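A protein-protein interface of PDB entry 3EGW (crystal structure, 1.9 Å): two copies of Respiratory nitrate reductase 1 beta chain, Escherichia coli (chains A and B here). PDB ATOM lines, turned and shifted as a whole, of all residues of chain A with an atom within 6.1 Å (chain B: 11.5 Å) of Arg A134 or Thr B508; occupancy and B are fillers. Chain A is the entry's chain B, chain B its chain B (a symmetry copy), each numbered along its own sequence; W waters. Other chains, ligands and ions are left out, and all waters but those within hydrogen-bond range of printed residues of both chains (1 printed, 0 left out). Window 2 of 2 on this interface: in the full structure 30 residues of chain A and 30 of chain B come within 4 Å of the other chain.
No position is printed for both chains.
The guanidinium group (NE) of Arg A127 lies within salt-bridge range of the side-chain carboxylate (OD2) of Asp A107. OD1 of Asp A107 lies within salt-bridge range of NH2 of Arg A134. The backbone carbonyl oxygen (O) of Arg A125 sits at hydrogen-bond distance from the guanidinium group (NH1) of Arg A134 (3.4 Å). The backbone carbonyl oxygen of Pro A126 sits at hydrogen-bond distance from the guanidinium group of Arg A134 (2.9 Å). The side-chain hydroxyl of Ser A128 lies within hydrogen-bond range of the backbone NH of Thr A131, 3.1 Å away. The backbone carbonyl oxygen (O) of Thr B505 is in hydrogen-bond range of the side-chain amino group (NZ) of Lys B507.
Thr A131 touches Val B504. N of Gly A132 touches CG1 of Val B504, 3.7 Å away. Thr B505 touches Gly A132 (O to CA, 3.5 Å). Gly A132 touches Ser B506 (O to C, 3.7 Å). Thr B508 touches Gly A132 (N to O, 3.8 Å). Glu A133 touches Lys B507 (OE2 to CG, 3.7 Å). Arg A134 touches Thr B508.
Hydrophobic or aromatic side chains of chain B within 4 Å of the printed part of chain A: Val B504. Along chain A the printed residues that touch a printed residue of chain B span positions 107 to 134.
Water W1 lies within hydrogen-bond range of OG of Ser B506 (2.5 Å), OD2 of Asp A107 (2.8 Å), OXT of Glu B509 (3.1 Å), OG1 of Thr B508 (3.2 Å) and NE of Arg A127 (3.3 Å).
The side-chain hydroxyl of Thr B508 lies within hydrogen-bond range of the side-chain carboxylate of Asp A107. The guanidinium group of Arg A127 sits close to the side-chain hydroxyl of Ser B506, 3.4 Å away. The guanidinium group (NE) of Arg A127 lies close to the side-chain hydroxyl (OG1) of Thr B508 (3.5 Å). The backbone carbonyl oxygen (O) of Thr A131 lies within hydrogen-bond range of the side-chain amino group (NZ) of Lys B507, at 2.8 Å. N of Lys B507 is in hydrogen-bond range of O of Gly A132.
Of the printed residues of chain B, Asp A107 touches Thr B508. No residue of chain B comes within 4 Å of Arg A125. Printed residues of chain B within 4 Å of Arg A127: Ser B506 (3.3 Å) and Thr B508 (3.5 Å). Of the printed residues of chain B, Thr A131 touches Val B504 (3.6 Å) and Lys B507 (2.8 Å). Of chain B, only Lys B507 (3.7 Å) comes within 4 Å of Glu A133. Printed residues of chain A within 4 Å of Val B504: Thr A131 (3.6 Å) and Gly A132 (3.7 Å). Of the printed residues of chain A, Thr B505 touches Gly A132. Printed residues of chain A within 4 Å of Ser B506: Arg A127 (3.3 Å) and Gly A132 (3.7 Å). Printed residues of chain A within 4 Å of Lys B507: Thr A131 (2.8 Å), Gly A132 (2.8 Å) and Glu A133 (3.7 Å). Printed residues of chain A within 4 Å of Thr B508: Asp A107, Arg A127, Gly A132 and Arg A134. The nearest residue of chain B that does not touch Arg A134 is Lys B507 (5.7 Å).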
ATOM      1  N   ASP A 107      -8.525  29.470 -10.805  1.00  0.00           N
ATOM      2  CA  ASP A 107      -7.872  30.768 -10.706  1.00  0.00           C
ATOM      3  C   ASP A 107      -7.789  31.431 -12.081  1.00  0.00           C
ATOM      4  O   ASP A 107      -6.706  31.589 -12.641  1.00  0.00           O
ATOM      5  CB  ASP A 107      -6.476  30.599 -10.095  1.00  0.00           C
ATOM      6  CG  ASP A 107      -6.523  30.378  -8.591  1.00  0.00           C
ATOM      7  OD1 ASP A 107      -5.582  29.773  -8.037  1.00  0.00           O
ATOM      8  OD2 ASP A 107      -7.499  30.824  -7.960  1.00  0.00           O
ATOM      9  N   ALA A 124      -5.113  28.373 -15.491  1.00  0.00           N
ATOM     10  CA  ALA A 124      -6.002  28.528 -14.344  1.00  0.00           C
ATOM     11  C   ALA A 124      -6.141  27.182 -13.642  1.00  0.00           C
ATOM     12  O   ALA A 124      -6.798  26.280 -14.158  1.00  0.00           O
ATOM     13  CB  ALA A 124      -7.373  29.021 -14.802  1.00  0.00           C
ATOM     14  N   ARG A 125      -5.524  27.049 -12.470  1.00  0.00           N
ATOM     15  CA  ARG A 125      -5.581  25.798 -11.709  1.00  0.00           C
ATOM     16  C   ARG A 125      -6.753  25.773 -10.734  1.00  0.00           C
ATOM     17  O   ARG A 125      -7.253  26.820 -10.326  1.00  0.00           O
ATOM     18  CB  ARG A 125      -4.270  25.582 -10.942  1.00  0.00           C
ATOM     19  CG  ARG A 125      -3.061  25.342 -11.844  1.00  0.00           C
ATOM     20  CD  ARG A 125      -1.769  25.199 -11.038  1.00  0.00           C
ATOM     21  NE  ARG A 125      -1.732  23.969 -10.251  1.00  0.00           N
ATOM     22  CZ  ARG A 125      -0.691  23.582  -9.516  1.00  0.00           C
ATOM     23  NH1 ARG A 125      -0.744  22.449  -8.835  1.00  0.00           N
ATOM     24  NH2 ARG A 125       0.404  24.328  -9.462  1.00  0.00           N
ATOM     25  N   PRO A 126      -7.208  24.568 -10.350  1.00  0.00           N
ATOM     26  CA  PRO A 126      -8.329  24.425  -9.419  1.00  0.00           C
ATOM     27  C   PRO A 126      -8.004  24.801  -7.981  1.00  0.00           C
ATOM     28  O   PRO A 126      -6.874  24.648  -7.515  1.00  0.00           O
ATOM     29  CB  PRO A 126      -8.714  22.953  -9.559  1.00  0.00           C
ATOM     30  CG  PRO A 126      -7.402  22.295  -9.869  1.00  0.00           C
ATOM     31  CD  PRO A 126      -6.793  23.254 -10.874  1.00  0.00           C
ATOM     32  N   ARG A 127      -9.023  25.291  -7.289  1.00  0.00           N
ATOM     33  CA  ARG A 127      -8.915  25.703  -5.897  1.00  0.00           C
ATOM     34  C   ARG A 127     -10.185  25.253  -5.189  1.00  0.00           C
ATOM     35  O   ARG A 127     -11.270  25.275  -5.766  1.00  0.00           O
ATOM     36  CB  ARG A 127      -8.769  27.228  -5.814  1.00  0.00           C
ATOM     37  CG  ARG A 127      -9.089  27.840  -4.458  1.00  0.00           C
ATOM     38  CD  ARG A 127      -8.687  29.314  -4.433  1.00  0.00           C
ATOM     39  NE  ARG A 127      -9.020  29.984  -5.686  1.00  0.00           N
ATOM     40  CZ  ARG A 127     -10.249  30.344  -6.048  1.00  0.00           C
ATOM     41  NH1 ARG A 127     -11.274  30.110  -5.244  1.00  0.00           N
ATOM     42  NH2 ARG A 127     -10.454  30.904  -7.235  1.00  0.00           N
ATOM     43  N   SER A 128     -10.043  24.836  -3.940  1.00  0.00           N
ATOM     44  CA  SER A 128     -11.185  24.378  -3.169  1.00  0.00           C
ATOM     45  C   SER A 128     -12.070  25.518  -2.669  1.00  0.00           C
ATOM     46  O   SER A 128     -11.571  26.540  -2.180  1.00  0.00           O
ATOM     47  CB  SER A 128     -10.704  23.556  -1.975  1.00  0.00           C
ATOM     48  OG  SER A 128     -11.768  23.306  -1.078  1.00  0.00           O
ATOM     49  N   THR A 131     -11.765  25.164   1.415  1.00  0.00           N
ATOM     50  CA  THR A 131     -10.571  25.647   2.107  1.00  0.00           C
ATOM     51  C   THR A 131      -9.878  26.834   1.444  1.00  0.00           C
ATOM     52  O   THR A 131      -9.087  27.530   2.085  1.00  0.00           O
ATOM     53  CB  THR A 131      -9.522  24.529   2.233  1.00  0.00           C
ATOM     54  OG1 THR A 131      -8.983  24.244   0.938  1.00  0.00           O
ATOM     55  CG2 THR A 131     -10.154  23.258   2.800  1.00  0.00           C
ATOM     56  N   GLY A 132     -10.164  27.056   0.165  1.00  0.00           N
ATOM     57  CA  GLY A 132      -9.530  28.144  -0.554  1.00  0.00           C
ATOM     58  C   GLY A 132      -8.121  27.766  -0.991  1.00  0.00           C
ATOM     59  O   GLY A 132      -7.402  28.584  -1.563  1.00  0.00           O
ATOM     60  N   GLU A 133      -7.729  26.520  -0.726  1.00  0.00           N
ATOM     61  CA  GLU A 133      -6.391  26.040  -1.074  1.00  0.00           C
ATOM     62  C   GLU A 133      -6.303  25.481  -2.486  1.00  0.00           C
ATOM     63  O   GLU A 133      -7.304  25.076  -3.081  1.00  0.00           O
ATOM     64  CB  GLU A 133      -5.945  24.931  -0.110  1.00  0.00           C
ATOM     65  CG  GLU A 133      -5.983  25.279   1.371  1.00  0.00           C
ATOM     66  CD  GLU A 133      -4.819  26.143   1.813  1.00  0.00           C
ATOM     67  OE1 GLU A 133      -3.905  26.388   0.994  1.00  0.00           O
ATOM     68  OE2 GLU A 133      -4.816  26.572   2.989  1.00  0.00           O
ATOM     69  N   ARG A 134      -5.084  25.448  -3.013  1.00  0.00           N
ATOM     70  CA  ARG A 134      -4.849  24.890  -4.332  1.00  0.00           C
ATOM     71  C   ARG A 134      -5.191  23.405  -4.258  1.00  0.00           C
ATOM     72  O   ARG A 134      -4.928  22.749  -3.250  1.00  0.00           O
ATOM     73  CB  ARG A 134      -3.372  25.048  -4.715  1.00  0.00           C
ATOM     74  CG  ARG A 134      -2.916  24.179  -5.889  1.00  0.00           C
ATOM     75  CD  ARG A 134      -3.446  24.690  -7.223  1.00  0.00           C
ATOM     76  NE  ARG A 134      -2.960  26.034  -7.523  1.00  0.00           N
ATOM     77  CZ  ARG A 134      -3.748  27.076  -7.759  1.00  0.00           C
ATOM     78  NH1 ARG A 134      -5.069  26.929  -7.728  1.00  0.00           N
ATOM     79  NH2 ARG A 134      -3.221  28.265  -8.030  1.00  0.00           N
ATOM     80  N   MET A 135      -5.803  22.886  -5.314  1.00  0.00           N
ATOM     81  CA  MET A 135      -6.126  21.471  -5.389  1.00  0.00           C
ATOM     82  C   MET A 135      -5.157  20.914  -6.424  1.00  0.00           C
ATOM     83  O   MET A 135      -5.024  21.475  -7.509  1.00  0.00           O
ATOM     84  CB  MET A 135      -7.571  21.265  -5.853  1.00  0.00           C
ATOM     85  CG  MET A 135      -8.614  21.681  -4.819  1.00  0.00           C
ATOM     86  SD  MET A 135     -10.298  21.600  -5.454  1.00  0.00           S
ATOM     87  CE  MET A 135     -10.548  19.842  -5.553  1.00  0.00           C
ATOM     88  N   ALA A 136      -4.459  19.838  -6.078  1.00  0.00           N
ATOM     89  CA  ALA A 136      -3.505  19.233  -6.998  1.00  0.00           C
ATOM     90  C   ALA A 136      -4.257  18.637  -8.177  1.00  0.00           C
ATOM     91  O   ALA A 136      -3.790  18.682  -9.313  1.00  0.00           O
ATOM     92  CB  ALA A 136      -2.706  18.153  -6.283  1.00  0.00           C
ATOM     93  N   VAL B 504     -14.975  32.015   2.787  1.00  0.00           N
ATOM     94  CA  VAL B 504     -13.750  31.235   2.637  1.00  0.00           C
ATOM     95  C   VAL B 504     -12.838  31.970   1.660  1.00  0.00           C
ATOM     96  O   VAL B 504     -13.087  31.992   0.458  1.00  0.00           O
ATOM     97  CB  VAL B 504     -14.041  29.818   2.104  1.00  0.00           C
ATOM     98  CG1 VAL B 504     -12.731  29.067   1.863  1.00  0.00           C
ATOM     99  CG2 VAL B 504     -14.905  29.060   3.105  1.00  0.00           C
ATOM    100  N   THR B 505     -11.783  32.575   2.193  1.00  0.00           N
ATOM    101  CA  THR B 505     -10.845  33.335   1.378  1.00  0.00           C
ATOM    102  C   THR B 505      -9.955  32.458   0.511  1.00  0.00           C
ATOM    103  O   THR B 505      -9.586  31.352   0.894  1.00  0.00           O
ATOM    104  CB  THR B 505      -9.928  34.194   2.257  1.00  0.00           C
ATOM    105  OG1 THR B 505      -9.196  33.340   3.144  1.00  0.00           O
ATOM    106  CG2 THR B 505     -10.739  35.193   3.068  1.00  0.00           C
ATOM    107  N   SER B 506      -9.618  32.955  -0.671  1.00  0.00           N
ATOM    108  CA  SER B 506      -8.734  32.214  -1.555  1.00  0.00           C
ATOM    109  C   SER B 506      -7.358  32.272  -0.919  1.00  0.00           C
ATOM    110  O   SER B 506      -6.942  33.329  -0.449  1.00  0.00           O
ATOM    111  CB  SER B 506      -8.668  32.867  -2.932  1.00  0.00           C
ATOM    112  OG  SER B 506      -7.565  32.346  -3.652  1.00  0.00           O
ATOM    113  N   LYS B 507      -6.655  31.147  -0.894  1.00  0.00           N
ATOM    114  CA  LYS B 507      -5.323  31.119  -0.307  1.00  0.00           C
ATOM    115  C   LYS B 507      -4.262  31.109  -1.407  1.00  0.00           C
ATOM    116  O   LYS B 507      -3.062  31.102  -1.125  1.00  0.00           O
ATOM    117  CB  LYS B 507      -5.153  29.880   0.578  1.00  0.00           C
ATOM    118  CG  LYS B 507      -6.278  29.645   1.585  1.00  0.00           C
ATOM    119  CD  LYS B 507      -6.480  30.833   2.515  1.00  0.00           C
ATOM    120  CE  LYS B 507      -7.460  30.493   3.638  1.00  0.00           C
ATOM    121  NZ  LYS B 507      -8.821  30.112   3.139  1.00  0.00           N
ATOM    122  N   THR B 508      -4.711  31.109  -2.659  1.00  0.00           N
ATOM    123  CA  THR B 508      -3.805  31.088  -3.805  1.00  0.00           C
ATOM    124  C   THR B 508      -3.621  32.495  -4.369  1.00  0.00           C
ATOM    125  O   THR B 508      -3.200  32.668  -5.516  1.00  0.00           O
ATOM    126  CB  THR B 508      -4.338  30.147  -4.918  1.00  0.00           C
ATOM    127  OG1 THR B 508      -5.599  30.631  -5.397  1.00  0.00           O
ATOM    128  CG2 THR B 508      -4.523  28.734  -4.373  1.00  0.00           C
ATOM    129  N   GLU B 509      -3.937  33.484  -3.536  1.00  0.00           N
ATOM    130  CA  GLU B 509      -3.833  34.903  -3.874  1.00  0.00           C
ATOM    131  C   GLU B 509      -5.035  35.385  -4.675  1.00  0.00           C
ATOM    132  O   GLU B 509      -5.754  36.273  -4.169  1.00  0.00           O
ATOM    133  CB  GLU B 509      -2.543  35.182  -4.650  1.00  0.00           C
ATOM    134  CG  GLU B 509      -2.425  36.606  -5.167  1.00  0.00           C
ATOM    135  CD  GLU B 509      -1.123  36.849  -5.899  1.00  0.00           C
ATOM    136  OE1 GLU B 509      -0.055  36.794  -5.252  1.00  0.00           O
ATOM    137  OE2 GLU B 509      -1.167  37.092  -7.124  1.00  0.00           O
ATOM    138  OXT GLU B 509      -5.247  34.867  -5.793  1.00  0.00           O
HETATM  139  O   HOH W   1      -7.631  32.983  -6.112  1.00  0.00           O
